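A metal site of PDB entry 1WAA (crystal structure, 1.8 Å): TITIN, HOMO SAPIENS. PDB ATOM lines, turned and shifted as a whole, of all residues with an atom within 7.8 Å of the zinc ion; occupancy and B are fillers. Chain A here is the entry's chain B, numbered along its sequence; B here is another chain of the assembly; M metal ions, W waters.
The side-chain carboxylate (OE2) of Glu 52 is in salt-bridge range of the side-chain amino group (NZ) of Lys 59 of chain B, 2.7 Å away. N of Glu 52 is in hydrogen-bond range of O of Ile 63, 2.8 Å away. The side-chain carboxylate (OE1) of Glu 26 of chain B lies close to the side-chain amino group (NZ) of Lys 59 of chain B, at 3.7 Å. OH of Tyr 13 of chain B is in hydrogen-bond range of OE2 of Glu 26 of chain B (3.1 Å). OE2 of Glu 26 of chain B lies within hydrogen-bond range of NE2 of His 24 of chain B, 2.9 Å away. N of His 65 lies within hydrogen-bond range of O of Asp 50 (2.8 Å). NZ of Lys 59 of chain B lies within salt-bridge range of OE2 of Glu 28 of chain B, 3.0 Å away.
Merely in contact with the zinc ion: Lys 59 of chain B (3.7 Å). Of the 18 residues printed, 4 come within 4 Å of the zinc ion. Along chain A the residues within 4 Å of the zinc ion span positions 52 to 65. The nearest printed residue that does not touch the zinc ion is Ile 63 (4.1 Å).
The zinc ion is bound by OE1 of Glu 52, OE1 of Glu 26 of chain B, water W1 and NE2 of His 65. The zinc ion has four donor atoms within binding distance.
Water W1 bridges the side-chain carboxylate of Glu 52 (3.1 Å) and the side-chain amino group of Lys 59 of chain B (3.2 Å).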
ATOM      1  N   THR A  22      23.021   9.404 -35.954  1.00  0.00           N
ATOM      2  CA  THR A  22      23.819   8.283 -35.472  1.00  0.00           C
ATOM      3  C   THR A  22      23.140   6.923 -35.651  1.00  0.00           C
ATOM      4  O   THR A  22      21.904   6.797 -35.552  1.00  0.00           O
ATOM      5  CB  THR A  22      24.395   8.499 -34.024  1.00  0.00           C
ATOM      6  OG1 THR A  22      23.944   7.500 -33.091  1.00  0.00           O
ATOM      7  CG2 THR A  22      24.139   9.829 -33.466  1.00  0.00           C
ATOM      8  N   SER A  48      37.001   6.280 -31.707  1.00  0.00           N
ATOM      9  CA  SER A  48      37.155   7.736 -31.776  1.00  0.00           C
ATOM     10  C   SER A  48      35.842   8.366 -31.279  1.00  0.00           C
ATOM     11  O   SER A  48      34.887   7.629 -30.996  1.00  0.00           O
ATOM     12  CB  SER A  48      37.530   8.200 -33.185  1.00  0.00           C
ATOM     13  OG  SER A  48      36.406   8.136 -34.037  1.00  0.00           O
ATOM     14  N   PRO A  49      35.782   9.710 -31.095  1.00  0.00           N
ATOM     15  CA  PRO A  49      34.520  10.363 -30.696  1.00  0.00           C
ATOM     16  C   PRO A  49      33.283  10.017 -31.552  1.00  0.00           C
ATOM     17  O   PRO A  49      32.186   9.900 -30.989  1.00  0.00           O
ATOM     18  CB  PRO A  49      34.827  11.859 -30.771  1.00  0.00           C
ATOM     19  CG  PRO A  49      36.305  11.974 -30.905  1.00  0.00           C
ATOM     20  CD  PRO A  49      36.914  10.661 -31.170  1.00  0.00           C
ATOM     21  N   ASP A  50      33.453   9.828 -32.866  1.00  0.00           N
ATOM     22  CA  ASP A  50      32.359   9.476 -33.758  1.00  0.00           C
ATOM     23  C   ASP A  50      32.200   7.979 -33.999  1.00  0.00           C
ATOM     24  O   ASP A  50      31.279   7.545 -34.671  1.00  0.00           O
ATOM     25  CB  ASP A  50      32.585  10.161 -35.108  1.00  0.00           C
ATOM     26  CG  ASP A  50      32.336  11.652 -35.056  1.00  0.00           C
ATOM     27  OD1 ASP A  50      31.882  12.151 -34.000  1.00  0.00           O
ATOM     28  OD2 ASP A  50      32.582  12.341 -36.057  1.00  0.00           O
ATOM     29  N   CYS A  51      33.114   7.192 -33.447  1.00  0.00           N
ATOM     30  CA  CYS A  51      33.124   5.760 -33.638  1.00  0.00           C
ATOM     31  C   CYS A  51      33.395   5.076 -32.285  1.00  0.00           C
ATOM     32  O   CYS A  51      34.526   4.927 -31.888  1.00  0.00           O
ATOM     33  CB  CYS A  51      34.195   5.372 -34.660  1.00  0.00           C
ATOM     34  SG  CYS A  51      34.169   3.588 -35.038  1.00  0.00           S
ATOM     35  N   GLU A  52      32.336   4.666 -31.603  1.00  0.00           N
ATOM     36  CA  GLU A  52      32.471   4.197 -30.234  1.00  0.00           C
ATOM     37  C   GLU A  52      32.236   2.687 -30.226  1.00  0.00           C
ATOM     38  O   GLU A  52      31.219   2.215 -30.755  1.00  0.00           O
ATOM     39  CB  GLU A  52      31.508   4.954 -29.339  1.00  0.00           C
ATOM     40  CG  GLU A  52      31.883   6.423 -29.260  1.00  0.00           C
ATOM     41  CD  GLU A  52      30.882   7.335 -28.558  1.00  0.00           C
ATOM     42  OE1 GLU A  52      29.715   7.412 -28.964  1.00  0.00           O
ATOM     43  OE2 GLU A  52      31.274   8.068 -27.645  1.00  0.00           O
ATOM     44  N   ILE A  54      32.009  -0.646 -27.937  1.00  0.00           N
ATOM     45  CA  ILE A  54      31.529  -0.923 -26.592  1.00  0.00           C
ATOM     46  C   ILE A  54      31.449  -2.445 -26.354  1.00  0.00           C
ATOM     47  O   ILE A  54      30.995  -3.176 -27.215  1.00  0.00           O
ATOM     48  CB  ILE A  54      30.114  -0.273 -26.406  1.00  0.00           C
ATOM     49  CG1 ILE A  54      30.129   1.255 -26.701  1.00  0.00           C
ATOM     50  CG2 ILE A  54      29.527  -0.586 -25.051  1.00  0.00           C
ATOM     51  CD1 ILE A  54      30.853   2.084 -25.672  1.00  0.00           C
ATOM     52  N   ILE A  63      28.662   2.341 -32.045  1.00  0.00           N
ATOM     53  CA  ILE A  63      27.897   3.568 -32.215  1.00  0.00           C
ATOM     54  C   ILE A  63      28.670   4.414 -33.227  1.00  0.00           C
ATOM     55  O   ILE A  63      29.874   4.695 -33.021  1.00  0.00           O
ATOM     56  CB  ILE A  63      27.760   4.317 -30.865  1.00  0.00           C
ATOM     57  CG1 ILE A  63      26.945   3.461 -29.881  1.00  0.00           C
ATOM     58  CG2 ILE A  63      27.145   5.729 -31.046  1.00  0.00           C
ATOM     59  CD1 ILE A  63      26.770   4.077 -28.501  1.00  0.00           C
ATOM     60  N   LEU A  64      27.996   4.782 -34.310  1.00  0.00           N
ATOM     61  CA  LEU A  64      28.574   5.670 -35.364  1.00  0.00           C
ATOM     62  C   LEU A  64      27.874   7.019 -35.355  1.00  0.00           C
ATOM     63  O   LEU A  64      26.727   7.091 -35.724  1.00  0.00           O
ATOM     64  CB  LEU A  64      28.476   4.998 -36.747  1.00  0.00           C
ATOM     65  CG  LEU A  64      29.268   3.674 -36.886  1.00  0.00           C
ATOM     66  CD1 LEU A  64      29.001   2.896 -38.176  1.00  0.00           C
ATOM     67  CD2 LEU A  64      30.749   3.898 -36.769  1.00  0.00           C
ATOM     68  N   HIS A  65      28.547   8.086 -34.925  1.00  0.00           N
ATOM     69  CA  HIS A  65      27.924   9.401 -34.899  1.00  0.00           C
ATOM     70  C   HIS A  65      28.198  10.135 -36.207  1.00  0.00           C
ATOM     71  O   HIS A  65      29.205   9.848 -36.872  1.00  0.00           O
ATOM     72  CB  HIS A  65      28.437  10.266 -33.749  1.00  0.00           C
ATOM     73  CG  HIS A  65      27.984   9.813 -32.396  1.00  0.00           C
ATOM     74  ND1 HIS A  65      26.657   9.712 -32.042  1.00  0.00           N
ATOM     75  CD2 HIS A  65      28.694   9.478 -31.282  1.00  0.00           C
ATOM     76  CE1 HIS A  65      26.565   9.312 -30.787  1.00  0.00           C
ATOM     77  NE2 HIS A  65      27.785   9.166 -30.307  1.00  0.00           N
ATOM     78  N   LYS B  10      29.442  14.343 -21.465  1.00  0.00           N
ATOM     79  CA  LYS B  10      28.521  14.415 -22.604  1.00  0.00           C
ATOM     80  C   LYS B  10      27.136  13.972 -22.135  1.00  0.00           C
ATOM     81  O   LYS B  10      26.938  12.810 -21.774  1.00  0.00           O
ATOM     82  CB  LYS B  10      28.995  13.484 -23.726  1.00  0.00           C
ATOM     83  CG  LYS B  10      30.337  13.883 -24.322  1.00  0.00           C
ATOM     84  CD  LYS B  10      30.640  13.155 -25.614  1.00  0.00           C
ATOM     85  N   TYR B  13      20.905  13.079 -24.685  1.00  0.00           N
ATOM     86  CA  TYR B  13      20.229  13.906 -25.702  1.00  0.00           C
ATOM     87  C   TYR B  13      18.922  13.236 -26.102  1.00  0.00           C
ATOM     88  O   TYR B  13      18.759  12.026 -25.991  1.00  0.00           O
ATOM     89  CB  TYR B  13      21.118  14.163 -26.942  1.00  0.00           C
ATOM     90  CG  TYR B  13      21.731  12.907 -27.528  1.00  0.00           C
ATOM     91  CD1 TYR B  13      23.023  12.491 -27.153  1.00  0.00           C
ATOM     92  CD2 TYR B  13      21.016  12.110 -28.421  1.00  0.00           C
ATOM     93  CE1 TYR B  13      23.589  11.274 -27.680  1.00  0.00           C
ATOM     94  CE2 TYR B  13      21.561  10.934 -28.950  1.00  0.00           C
ATOM     95  CZ  TYR B  13      22.836  10.515 -28.578  1.00  0.00           C
ATOM     96  OH  TYR B  13      23.346   9.330 -29.098  1.00  0.00           O
ATOM     97  N   HIS B  24      18.116   4.513 -28.565  1.00  0.00           N
ATOM     98  CA  HIS B  24      19.230   4.369 -27.649  1.00  0.00           C
ATOM     99  C   HIS B  24      19.603   5.745 -27.089  1.00  0.00           C
ATOM    100  O   HIS B  24      19.532   6.777 -27.775  1.00  0.00           O
ATOM    101  CB  HIS B  24      20.421   3.614 -28.311  1.00  0.00           C
ATOM    102  CG  HIS B  24      21.590   4.445 -28.814  1.00  0.00           C
ATOM    103  ND1 HIS B  24      21.730   4.747 -30.161  1.00  0.00           N
ATOM    104  CD2 HIS B  24      22.659   4.996 -28.186  1.00  0.00           C
ATOM    105  CE1 HIS B  24      22.836   5.452 -30.318  1.00  0.00           C
ATOM    106  NE2 HIS B  24      23.410   5.619 -29.145  1.00  0.00           N
ATOM    107  N   GLU B  26      22.622   7.683 -24.468  1.00  0.00           N
ATOM    108  CA  GLU B  26      23.983   7.526 -23.997  1.00  0.00           C
ATOM    109  C   GLU B  26      24.460   8.774 -23.281  1.00  0.00           C
ATOM    110  O   GLU B  26      24.050   9.888 -23.578  1.00  0.00           O
ATOM    111  CB  GLU B  26      24.941   7.224 -25.160  1.00  0.00           C
ATOM    112  CG  GLU B  26      24.771   8.113 -26.373  1.00  0.00           C
ATOM    113  CD  GLU B  26      25.901   7.934 -27.359  1.00  0.00           C
ATOM    114  OE1 GLU B  26      27.068   8.340 -27.056  1.00  0.00           O
ATOM    115  OE2 GLU B  26      25.665   7.379 -28.469  1.00  0.00           O
ATOM    116  N   ILE B  27      25.318   8.547 -22.328  1.00  0.00           N
ATOM    117  CA  ILE B  27      25.897   9.620 -21.552  1.00  0.00           C
ATOM    118  C   ILE B  27      27.333   9.218 -21.246  1.00  0.00           C
ATOM    119  O   ILE B  27      27.624   8.044 -21.066  1.00  0.00           O
ATOM    120  CB  ILE B  27      25.072   9.865 -20.262  1.00  0.00           C
ATOM    121  CG1 ILE B  27      25.753  10.884 -19.320  1.00  0.00           C
ATOM    122  CG2 ILE B  27      24.858   8.572 -19.471  1.00  0.00           C
ATOM    123  CD1 ILE B  27      24.824  11.422 -18.235  1.00  0.00           C
ATOM    124  N   GLU B  28      28.212  10.191 -21.214  1.00  0.00           N
ATOM    125  CA  GLU B  28      29.609   9.940 -20.879  1.00  0.00           C
ATOM    126  C   GLU B  28      29.944  10.696 -19.614  1.00  0.00           C
ATOM    127  O   GLU B  28      29.794  11.922 -19.532  1.00  0.00           O
ATOM    128  CB  GLU B  28      30.528  10.399 -21.993  1.00  0.00           C
ATOM    129  CG  GLU B  28      31.989  10.073 -21.735  1.00  0.00           C
ATOM    130  CD  GLU B  28      32.870  10.430 -22.915  1.00  0.00           C
ATOM    131  OE1 GLU B  28      33.776  11.329 -22.792  1.00  0.00           O
ATOM    132  OE2 GLU B  28      32.671   9.837 -24.020  1.00  0.00           O
ATOM    133  N   LYS B  59      31.316   5.453 -20.388  1.00  0.00           N
ATOM    134  CA  LYS B  59      30.056   5.477 -21.139  1.00  0.00           C
ATOM    135  C   LYS B  59      28.950   4.605 -20.513  1.00  0.00           C
ATOM    136  O   LYS B  59      29.181   3.472 -20.109  1.00  0.00           O
ATOM    137  CB  LYS B  59      30.289   4.959 -22.568  1.00  0.00           C
ATOM    138  CG  LYS B  59      31.426   5.694 -23.279  1.00  0.00           C
ATOM    139  CD  LYS B  59      30.981   6.324 -24.617  1.00  0.00           C
ATOM    140  CE  LYS B  59      29.940   7.430 -24.434  1.00  0.00           C
ATOM    141  NZ  LYS B  59      30.236   8.641 -25.252  1.00  0.00           N
ATOM    142  N   ILE B  61      24.993   3.383 -21.486  1.00  0.00           N
ATOM    143  CA  ILE B  61      24.066   3.271 -22.621  1.00  0.00           C
ATOM    144  C   ILE B  61      22.766   2.558 -22.227  1.00  0.00           C
ATOM    145  O   ILE B  61      22.788   1.602 -21.446  1.00  0.00           O
ATOM    146  CB  ILE B  61      24.754   2.472 -23.734  1.00  0.00           C
ATOM    147  CG1 ILE B  61      25.853   3.304 -24.417  1.00  0.00           C
ATOM    148  CG2 ILE B  61      23.755   1.999 -24.795  1.00  0.00           C
ATOM    149  CD1 ILE B  61      26.837   2.474 -25.215  1.00  0.00           C
HETATM  150 ZN    ZN M   1      28.459   8.600 -28.465  1.00  0.00          ZN
HETATM  151  O   HOH W   1      29.175  10.349 -27.716  1.00  0.00           O
